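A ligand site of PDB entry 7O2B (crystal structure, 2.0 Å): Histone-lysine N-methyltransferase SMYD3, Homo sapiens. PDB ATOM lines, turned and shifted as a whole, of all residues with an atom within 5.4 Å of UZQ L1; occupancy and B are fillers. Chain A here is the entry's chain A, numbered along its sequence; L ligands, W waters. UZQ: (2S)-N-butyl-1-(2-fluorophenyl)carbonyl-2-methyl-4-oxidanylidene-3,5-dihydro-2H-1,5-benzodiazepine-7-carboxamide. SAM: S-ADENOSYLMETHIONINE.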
ATOM      1  N   CYS A 180      26.933 -15.947   1.606  1.00  0.00           N
ATOM      2  CA  CYS A 180      25.906 -16.915   1.328  1.00  0.00           C
ATOM      3  C   CYS A 180      26.264 -18.358   1.721  1.00  0.00           C
ATOM      4  O   CYS A 180      25.577 -19.267   1.303  1.00  0.00           O
ATOM      5  CB  CYS A 180      25.511 -16.841  -0.125  1.00  0.00           C
ATOM      6  SG  CYS A 180      26.728 -17.433  -1.314  1.00  0.00           S
ATOM      7  N   ASN A 181      27.327 -18.551   2.488  1.00  0.00           N
ATOM      8  CA  ASN A 181      27.693 -19.895   3.020  1.00  0.00           C
ATOM      9  C   ASN A 181      28.022 -19.923   4.523  1.00  0.00           C
ATOM     10  O   ASN A 181      28.590 -20.897   5.009  1.00  0.00           O
ATOM     11  CB  ASN A 181      28.853 -20.491   2.228  1.00  0.00           C
ATOM     12  CG  ASN A 181      28.474 -20.795   0.807  1.00  0.00           C
ATOM     13  OD1 ASN A 181      27.846 -21.846   0.545  1.00  0.00           O
ATOM     14  ND2 ASN A 181      28.820 -19.910  -0.126  1.00  0.00           N
ATOM     15  N   SER A 182      27.695 -18.864   5.244  1.00  0.00           N
ATOM     16  CA  SER A 182      27.938 -18.841   6.680  1.00  0.00           C
ATOM     17  C   SER A 182      26.833 -19.530   7.431  1.00  0.00           C
ATOM     18  O   SER A 182      25.689 -19.172   7.280  1.00  0.00           O
ATOM     19  CB  SER A 182      28.015 -17.435   7.202  1.00  0.00           C
ATOM     20  OG  SER A 182      29.214 -16.868   6.746  1.00  0.00           O
ATOM     21  N   PHE A 183      27.212 -20.474   8.264  1.00  0.00           N
ATOM     22  CA  PHE A 183      26.325 -21.131   9.179  1.00  0.00           C
ATOM     23  C   PHE A 183      26.292 -20.459  10.560  1.00  0.00           C
ATOM     24  O   PHE A 183      27.326 -20.235  11.150  1.00  0.00           O
ATOM     25  CB  PHE A 183      26.730 -22.603   9.300  1.00  0.00           C
ATOM     26  CG  PHE A 183      26.408 -23.393   8.073  1.00  0.00           C
ATOM     27  CD1 PHE A 183      25.250 -24.153   8.002  1.00  0.00           C
ATOM     28  CD2 PHE A 183      27.234 -23.362   6.990  1.00  0.00           C
ATOM     29  CE1 PHE A 183      24.917 -24.876   6.863  1.00  0.00           C
ATOM     30  CE2 PHE A 183      26.922 -24.070   5.833  1.00  0.00           C
ATOM     31  CZ  PHE A 183      25.752 -24.837   5.764  1.00  0.00           C
ATOM     32  N   THR A 184      25.100 -20.136  11.066  1.00  0.00           N
ATOM     33  CA  THR A 184      24.981 -19.724  12.434  1.00  0.00           C
ATOM     34  C   THR A 184      24.979 -20.925  13.423  1.00  0.00           C
ATOM     35  O   THR A 184      24.148 -21.839  13.309  1.00  0.00           O
ATOM     36  CB  THR A 184      23.723 -18.889  12.655  1.00  0.00           C
ATOM     37  OG1 THR A 184      23.803 -17.722  11.847  1.00  0.00           O
ATOM     38  CG2 THR A 184      23.608 -18.461  14.118  1.00  0.00           C
ATOM     39  N   ILE A 185      25.900 -20.912  14.379  1.00  0.00           N
ATOM     40  CA  ILE A 185      26.087 -22.028  15.324  1.00  0.00           C
ATOM     41  C   ILE A 185      25.309 -21.599  16.571  1.00  0.00           C
ATOM     42  O   ILE A 185      25.558 -20.507  17.101  1.00  0.00           O
ATOM     43  CB  ILE A 185      27.558 -22.240  15.640  1.00  0.00           C
ATOM     44  CG1 ILE A 185      28.342 -22.582  14.377  1.00  0.00           C
ATOM     45  CG2 ILE A 185      27.743 -23.406  16.596  1.00  0.00           C
ATOM     46  CD1 ILE A 185      29.836 -22.383  14.552  1.00  0.00           C
ATOM     47  N   CYS A 186      24.310 -22.389  16.947  1.00  0.00           N
ATOM     48  CA  CYS A 186      23.640 -22.210  18.225  1.00  0.00           C
ATOM     49  C   CYS A 186      24.046 -23.253  19.256  1.00  0.00           C
ATOM     50  O   CYS A 186      24.364 -24.379  18.914  1.00  0.00           O
ATOM     51  CB  CYS A 186      22.112 -22.225  18.074  1.00  0.00           C
ATOM     52  SG  CYS A 186      21.395 -21.006  16.922  1.00  0.00           S
ATOM     53  N   MET A 190      19.613 -23.330  21.942  1.00  0.00           N
ATOM     54  CA  MET A 190      19.294 -22.548  20.741  1.00  0.00           C
ATOM     55  C   MET A 190      19.626 -21.067  20.707  1.00  0.00           C
ATOM     56  O   MET A 190      19.131 -20.351  19.850  1.00  0.00           O
ATOM     57  CB  MET A 190      17.885 -22.814  20.294  1.00  0.00           C
ATOM     58  CG  MET A 190      17.673 -24.243  19.814  1.00  0.00           C
ATOM     59  SD  MET A 190      18.627 -24.462  18.294  1.00  0.00           S
ATOM     60  CE  MET A 190      18.382 -26.156  17.948  1.00  0.00           C
ATOM     61  N   GLU A 192      22.318 -18.138  19.760  1.00  0.00           N
ATOM     62  CA  GLU A 192      23.393 -17.978  18.782  1.00  0.00           C
ATOM     63  C   GLU A 192      24.686 -17.699  19.519  1.00  0.00           C
ATOM     64  O   GLU A 192      24.759 -16.797  20.331  1.00  0.00           O
ATOM     65  CB  GLU A 192      23.136 -16.824  17.808  1.00  0.00           C
ATOM     66  CG  GLU A 192      21.870 -17.029  17.011  1.00  0.00           C
ATOM     67  CD  GLU A 192      21.470 -15.840  16.116  1.00  0.00           C
ATOM     68  OE1 GLU A 192      22.300 -14.924  15.863  1.00  0.00           O
ATOM     69  OE2 GLU A 192      20.289 -15.831  15.689  1.00  0.00           O
ATOM     70  N   SER A 202      27.479 -26.997   2.703  1.00  0.00           N
ATOM     71  CA  SER A 202      27.074 -25.837   1.976  1.00  0.00           C
ATOM     72  C   SER A 202      26.389 -26.206   0.647  1.00  0.00           C
ATOM     73  O   SER A 202      25.790 -25.345   0.029  1.00  0.00           O
ATOM     74  CB  SER A 202      28.306 -24.978   1.631  1.00  0.00           C
ATOM     75  OG  SER A 202      28.565 -24.067   2.628  1.00  0.00           O
ATOM     76  N   ILE A 214      19.629 -29.328  10.295  1.00  0.00           N
ATOM     77  CA  ILE A 214      20.912 -29.251  10.989  1.00  0.00           C
ATOM     78  C   ILE A 214      20.813 -28.805  12.457  1.00  0.00           C
ATOM     79  O   ILE A 214      19.963 -27.961  12.817  1.00  0.00           O
ATOM     80  CB  ILE A 214      21.935 -28.326  10.323  1.00  0.00           C
ATOM     81  CG1 ILE A 214      21.438 -26.882  10.314  1.00  0.00           C
ATOM     82  CG2 ILE A 214      22.296 -28.842   8.955  1.00  0.00           C
ATOM     83  CD1 ILE A 214      22.497 -25.937   9.751  1.00  0.00           C
ATOM     84  N   VAL A 215      21.664 -29.407  13.271  1.00  0.00           N
ATOM     85  CA  VAL A 215      21.788 -29.059  14.670  1.00  0.00           C
ATOM     86  C   VAL A 215      23.245 -29.082  15.036  1.00  0.00           C
ATOM     87  O   VAL A 215      24.053 -29.827  14.445  1.00  0.00           O
ATOM     88  CB  VAL A 215      21.146 -30.030  15.654  1.00  0.00           C
ATOM     89  CG1 VAL A 215      19.657 -29.904  15.629  1.00  0.00           C
ATOM     90  CG2 VAL A 215      21.578 -31.482  15.394  1.00  0.00           C
ATOM     91  N   PHE A 216      23.558 -28.286  16.053  1.00  0.00           N
ATOM     92  CA  PHE A 216      24.968 -28.124  16.462  1.00  0.00           C
ATOM     93  C   PHE A 216      25.145 -28.616  17.880  1.00  0.00           C
ATOM     94  O   PHE A 216      24.275 -28.406  18.715  1.00  0.00           O
ATOM     95  CB  PHE A 216      25.401 -26.675  16.390  1.00  0.00           C
ATOM     96  CG  PHE A 216      25.425 -26.137  15.024  1.00  0.00           C
ATOM     97  CD1 PHE A 216      26.606 -26.218  14.240  1.00  0.00           C
ATOM     98  CD2 PHE A 216      24.302 -25.519  14.484  1.00  0.00           C
ATOM     99  CE1 PHE A 216      26.614 -25.734  12.925  1.00  0.00           C
ATOM    100  CE2 PHE A 216      24.323 -25.046  13.194  1.00  0.00           C
ATOM    101  CZ  PHE A 216      25.468 -25.148  12.418  1.00  0.00           C
ATOM    102  N   ILE A 237      17.288 -27.781   3.459  1.00  0.00           N
ATOM    103  CA  ILE A 237      17.167 -27.310   4.818  1.00  0.00           C
ATOM    104  C   ILE A 237      16.609 -25.916   4.739  1.00  0.00           C
ATOM    105  O   ILE A 237      16.724 -25.260   3.674  1.00  0.00           O
ATOM    106  CB  ILE A 237      18.502 -27.243   5.570  1.00  0.00           C
ATOM    107  CG1 ILE A 237      19.531 -26.469   4.773  1.00  0.00           C
ATOM    108  CG2 ILE A 237      19.083 -28.627   5.811  1.00  0.00           C
ATOM    109  CD1 ILE A 237      20.653 -25.975   5.589  1.00  0.00           C
ATOM    110  N   CYS A 238      16.024 -25.421   5.837  1.00  0.00           N
ATOM    111  CA  CYS A 238      15.515 -24.061   5.816  1.00  0.00           C
ATOM    112  C   CYS A 238      16.618 -23.148   6.363  1.00  0.00           C
ATOM    113  O   CYS A 238      17.110 -23.319   7.450  1.00  0.00           O
ATOM    114  CB  CYS A 238      14.206 -23.981   6.620  1.00  0.00           C
ATOM    115  SG  CYS A 238      13.572 -22.292   6.587  1.00  0.00           S
ATOM    116  N   TYR A 239      17.078 -22.229   5.542  1.00  0.00           N
ATOM    117  CA  TYR A 239      18.176 -21.343   5.890  1.00  0.00           C
ATOM    118  C   TYR A 239      17.741 -20.299   6.940  1.00  0.00           C
ATOM    119  O   TYR A 239      18.603 -19.638   7.584  1.00  0.00           O
ATOM    120  CB  TYR A 239      18.639 -20.560   4.660  1.00  0.00           C
ATOM    121  CG  TYR A 239      19.352 -21.279   3.531  1.00  0.00           C
ATOM    122  CD1 TYR A 239      19.635 -22.613   3.571  1.00  0.00           C
ATOM    123  CD2 TYR A 239      19.801 -20.555   2.424  1.00  0.00           C
ATOM    124  CE1 TYR A 239      20.314 -23.241   2.518  1.00  0.00           C
ATOM    125  CE2 TYR A 239      20.471 -21.153   1.369  1.00  0.00           C
ATOM    126  CZ  TYR A 239      20.730 -22.513   1.421  1.00  0.00           C
ATOM    127  OH  TYR A 239      21.455 -23.103   0.410  1.00  0.00           O
ATOM    128  N   LEU A 240      16.424 -20.133   7.085  1.00  0.00           N
ATOM    129  CA  LEU A 240      15.860 -19.023   7.845  1.00  0.00           C
ATOM    130  C   LEU A 240      15.068 -19.401   9.118  1.00  0.00           C
ATOM    131  O   LEU A 240      14.523 -20.498   9.256  1.00  0.00           O
ATOM    132  CB  LEU A 240      14.924 -18.252   6.899  1.00  0.00           C
ATOM    133  CG  LEU A 240      15.360 -17.934   5.476  1.00  0.00           C
ATOM    134  CD1 LEU A 240      14.288 -17.185   4.720  1.00  0.00           C
ATOM    135  CD2 LEU A 240      16.602 -17.066   5.570  1.00  0.00           C
ATOM    136  N   ASP A 241      14.957 -18.451  10.006  1.00  0.00           N
ATOM    137  CA  ASP A 241      14.033 -18.529  11.126  1.00  0.00           C
ATOM    138  C   ASP A 241      12.652 -18.825  10.617  1.00  0.00           C
ATOM    139  O   ASP A 241      12.219 -18.247   9.651  1.00  0.00           O
ATOM    140  CB  ASP A 241      14.086 -17.156  11.791  1.00  0.00           C
ATOM    141  CG  ASP A 241      13.186 -17.003  13.012  1.00  0.00           C
ATOM    142  OD1 ASP A 241      12.615 -17.955  13.515  1.00  0.00           O
ATOM    143  OD2 ASP A 241      13.051 -15.865  13.467  1.00  0.00           O
ATOM    144  N   TYR A 257      21.216 -14.329  -0.239  1.00  0.00           N
ATOM    145  CA  TYR A 257      21.406 -15.518  -1.058  1.00  0.00           C
ATOM    146  C   TYR A 257      21.152 -15.346  -2.563  1.00  0.00           C
ATOM    147  O   TYR A 257      21.406 -16.264  -3.363  1.00  0.00           O
ATOM    148  CB  TYR A 257      20.548 -16.650  -0.521  1.00  0.00           C
ATOM    149  CG  TYR A 257      20.940 -17.015   0.885  1.00  0.00           C
ATOM    150  CD1 TYR A 257      22.074 -17.774   1.116  1.00  0.00           C
ATOM    151  CD2 TYR A 257      20.205 -16.543   1.992  1.00  0.00           C
ATOM    152  CE1 TYR A 257      22.449 -18.105   2.384  1.00  0.00           C
ATOM    153  CE2 TYR A 257      20.579 -16.866   3.275  1.00  0.00           C
ATOM    154  CZ  TYR A 257      21.736 -17.639   3.462  1.00  0.00           C
ATOM    155  OH  TYR A 257      22.175 -18.014   4.716  1.00  0.00           O
ATOM    156  N   HIS A 366      11.200 -30.308  14.172  1.00  0.00           N
ATOM    157  CA  HIS A 366      12.070 -29.121  14.084  1.00  0.00           C
ATOM    158  C   HIS A 366      12.790 -28.979  15.429  1.00  0.00           C
ATOM    159  O   HIS A 366      12.108 -28.927  16.480  1.00  0.00           O
ATOM    160  CB  HIS A 366      11.231 -27.854  13.764  1.00  0.00           C
ATOM    161  CG  HIS A 366      12.044 -26.688  13.330  1.00  0.00           C
ATOM    162  ND1 HIS A 366      13.055 -26.163  14.105  1.00  0.00           N
ATOM    163  CD2 HIS A 366      12.053 -25.986  12.172  1.00  0.00           C
ATOM    164  CE1 HIS A 366      13.627 -25.155  13.459  1.00  0.00           C
ATOM    165  NE2 HIS A 366      13.043 -25.040  12.261  1.00  0.00           N
ATOM    166  N   PRO A 367      14.152 -28.899  15.418  1.00  0.00           N
ATOM    167  CA  PRO A 367      14.918 -28.862  16.624  1.00  0.00           C
ATOM    168  C   PRO A 367      14.576 -27.704  17.534  1.00  0.00           C
ATOM    169  O   PRO A 367      14.731 -27.836  18.737  1.00  0.00           O
ATOM    170  CB  PRO A 367      16.365 -28.776  16.119  1.00  0.00           C
ATOM    171  CG  PRO A 367      16.267 -28.178  14.769  1.00  0.00           C
ATOM    172  CD  PRO A 367      15.038 -28.862  14.246  1.00  0.00           C
ATOM    173  N   VAL A 368      14.147 -26.570  16.965  1.00  0.00           N
ATOM    174  CA  VAL A 368      13.780 -25.442  17.798  1.00  0.00           C
ATOM    175  C   VAL A 368      12.553 -25.753  18.636  1.00  0.00           C
ATOM    176  O   VAL A 368      12.483 -25.381  19.788  1.00  0.00           O
ATOM    177  CB  VAL A 368      13.578 -24.148  16.946  1.00  0.00           C
ATOM    178  CG1 VAL A 368      12.965 -22.998  17.774  1.00  0.00           C
ATOM    179  CG2 VAL A 368      14.922 -23.737  16.400  1.00  0.00           C
HETATM  180  C4  UZQ L   1      21.677 -22.300  11.415  1.00  0.00           C
HETATM  181  C5  UZQ L   1      21.087 -21.855  10.216  1.00  0.00           C
HETATM  182  C6  UZQ L   1      19.704 -21.645  10.213  1.00  0.00           C
HETATM  183  C7  UZQ L   1      21.982 -21.548   9.034  1.00  0.00           C
HETATM  184  C10 UZQ L   1      22.120 -20.670   6.680  1.00  0.00           C
HETATM  185  C13 UZQ L   1      24.476 -21.327   4.484  1.00  0.00           C
HETATM  186  C15 UZQ L   1      21.113 -23.908  14.442  1.00  0.00           C
HETATM  187  C17 UZQ L   1      18.618 -23.798  14.300  1.00  0.00           C
HETATM  188  C20 UZQ L   1      17.444 -24.502  13.635  1.00  0.00           C
HETATM  189  C21 UZQ L   1      18.200 -21.430  14.257  1.00  0.00           C
HETATM  190  C24 UZQ L   1      17.210 -19.471  13.072  1.00  0.00           C
HETATM  191  C26 UZQ L   1      18.565 -17.498  12.454  1.00  0.00           C
HETATM  192  C28 UZQ L   1      19.539 -19.349  13.587  1.00  0.00           C
HETATM  193  C12 UZQ L   1      23.006 -21.568   4.496  1.00  0.00           C
HETATM  194  C11 UZQ L   1      22.514 -21.899   5.897  1.00  0.00           C
HETATM  195  N9  UZQ L   1      21.397 -21.090   7.893  1.00  0.00           N
HETATM  196  O8  UZQ L   1      23.165 -21.400   9.283  1.00  0.00           O
HETATM  197  C1  UZQ L   1      18.916 -21.869  11.379  1.00  0.00           C
HETATM  198  C2  UZQ L   1      19.515 -22.306  12.562  1.00  0.00           C
HETATM  199  C3  UZQ L   1      20.886 -22.523  12.568  1.00  0.00           C
HETATM  200  N14 UZQ L   1      21.544 -22.934  13.670  1.00  0.00           N
HETATM  201  O19 UZQ L   1      21.766 -24.154  15.465  1.00  0.00           O
HETATM  202  C16 UZQ L   1      19.850 -24.653  14.056  1.00  0.00           C
HETATM  203  N18 UZQ L   1      18.729 -22.485  13.629  1.00  0.00           N
HETATM  204  O22 UZQ L   1      17.442 -21.538  15.227  1.00  0.00           O
HETATM  205  C23 UZQ L   1      18.322 -20.051  13.625  1.00  0.00           C
HETATM  206  C25 UZQ L   1      17.356 -18.209  12.504  1.00  0.00           C
HETATM  207  C27 UZQ L   1      19.669 -18.093  13.009  1.00  0.00           C
HETATM  208  F29 UZQ L   1      20.629 -19.880  14.128  1.00  0.00           F
HETATM  209  N   SAM L   2      23.516 -24.096  -4.762  1.00  0.00           N
HETATM  210  CA  SAM L   2      24.735 -23.826  -4.006  1.00  0.00           C
HETATM  211  C   SAM L   2      26.009 -24.162  -4.771  1.00  0.00           C
HETATM  212  O   SAM L   2      25.920 -24.338  -5.982  1.00  0.00           O
HETATM  213  OXT SAM L   2      27.109 -24.227  -4.179  1.00  0.00           O
HETATM  214  CB  SAM L   2      24.689 -24.586  -2.674  1.00  0.00           C
HETATM  215  CG  SAM L   2      23.849 -23.823  -1.625  1.00  0.00           C
HETATM  216  SD  SAM L   2      24.634 -22.473  -1.051  1.00  0.00           S
HETATM  217  CE  SAM L   2      24.786 -22.762   0.589  1.00  0.00           C
HETATM  218  C5' SAM L   2      23.585 -21.127  -1.183  1.00  0.00           C
HETATM  219  C4' SAM L   2      23.198 -20.701  -2.593  1.00  0.00           C
HETATM  220  O4' SAM L   2      22.525 -21.713  -3.288  1.00  0.00           O
HETATM  221  C3' SAM L   2      22.268 -19.465  -2.730  1.00  0.00           C
HETATM  222  O3' SAM L   2      22.916 -18.188  -2.507  1.00  0.00           O
HETATM  223  C2' SAM L   2      21.677 -19.643  -4.077  1.00  0.00           C
HETATM  224  O2' SAM L   2      22.630 -19.370  -5.122  1.00  0.00           O
HETATM  225  C1' SAM L   2      21.512 -21.149  -4.105  1.00  0.00           C
HETATM  226  N9  SAM L   2      20.184 -21.621  -3.606  1.00  0.00           N
HETATM  227  C8  SAM L   2      19.965 -22.228  -2.435  1.00  0.00           C
HETATM  228  N7  SAM L   2      18.685 -22.581  -2.306  1.00  0.00           N
HETATM  229  C5  SAM L   2      18.061 -22.193  -3.428  1.00  0.00           C
HETATM  230  C6  SAM L   2      16.708 -22.260  -3.969  1.00  0.00           C
HETATM  231  N6  SAM L   2      15.719 -22.819  -3.217  1.00  0.00           N
HETATM  232  N1  SAM L   2      16.480 -21.737  -5.238  1.00  0.00           N
HETATM  233  C2  SAM L   2      17.461 -21.220  -5.978  1.00  0.00           C
HETATM  234  N3  SAM L   2      18.731 -21.117  -5.535  1.00  0.00           N
HETATM  235  C4  SAM L   2      19.067 -21.565  -4.297  1.00  0.00           C
HETATM  236  O   HOH W   1      21.467 -26.444  16.871  1.00  0.00           O
HETATM  237  O   HOH W   2      23.854 -18.169   8.686  1.00  0.00           O
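Water W1 lies within hydrogen-bond range of an oxygen (O19) of UZQ L1 (2.7 Å), the backbone NH (N) of Phe 216 (2.9 Å) and the side-chain sulfur (SD) of Met 190 (3.7 Å).
Water W2 lies within hydrogen-bond range of O of Ser 182, OG1 of Thr 184 and O8 of UZQ L1.
O3' of SAM L2 is in hydrogen-bond range of O of Tyr 257 (2.6 Å).
A nitrogen (N14) of UZQ L1 lies within hydrogen-bond range of the backbone carbonyl oxygen (O) of Thr 184, at 2.8 Å.
The backbone carbonyl oxygen (O) of Tyr 239 lies within hydrogen-bond range of a nitrogen (N9) of UZQ L1, 3.2 Å away.
The backbone NH of Thr 184 is in hydrogen-bond range of an oxygen (O8) of UZQ L1 (2.9 Å).
N of Cys 186 sits close to O19 of UZQ L1, 3.4 Å away.
An oxygen (O19) of UZQ L1 lies close to the side-chain sulfur of Cys 186 (3.5 Å).
The side-chain sulfur (SG) of Cys 186 is in hydrogen-bond range of the backbone carbonyl oxygen (O) of Met 190 (3.8 Å).
N of Val 368 sits at hydrogen-bond distance from ND1 of His 366.
The side-chain amide oxygen (OD1) of Asn 181 is in hydrogen-bond range of the side-chain hydroxyl (OG) of Ser 202 (3.1 Å).
SG of Cys 180 lies within hydrogen-bond range of ND2 of Asn 181, at 3.5 Å.
O of Cys 180 touches C13 of UZQ L1, 3.9 Å away.
Asn 181 touches UZQ L1 (CA to C13, 3.8 Å).
Ser 182 touches UZQ L1 (O to C13, 3.7 Å).
Phe 183 touches UZQ L1 (CA to O8, 3.2 Å).
Glu 192 touches UZQ L1 (OE2 to C27, 3.6 Å).
Ile 214 touches UZQ L1.
CD2 of Phe 216 touches O19 of UZQ L1 (3.0 Å).
N of Asp 241 touches C25 of UZQ L1, at 3.5 Å.
Tyr 257 touches UZQ L1 (OH to C10, 3.3 Å).
His 366 touches UZQ L1 (CE1 to C20, 3.9 Å).
CG2 of Val 368 touches O22 of UZQ L1, at 3.5 Å.
Hydrophobic or aromatic side chains that line UZQ L1: Phe 183, Phe 216, Tyr 239, His 366 and Val 368.
Within 4 Å of UZQ L1: Cys 180, Asn 181, Ser 182, Phe 183, Thr 184, Cys 186, Glu 192, Ile 214, Phe 216, Tyr 239, Asp 241, Tyr 257, His 366 and Val 368.
Along chain A the residues within 4 Å of UZQ L1 span positions 180 to 368.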
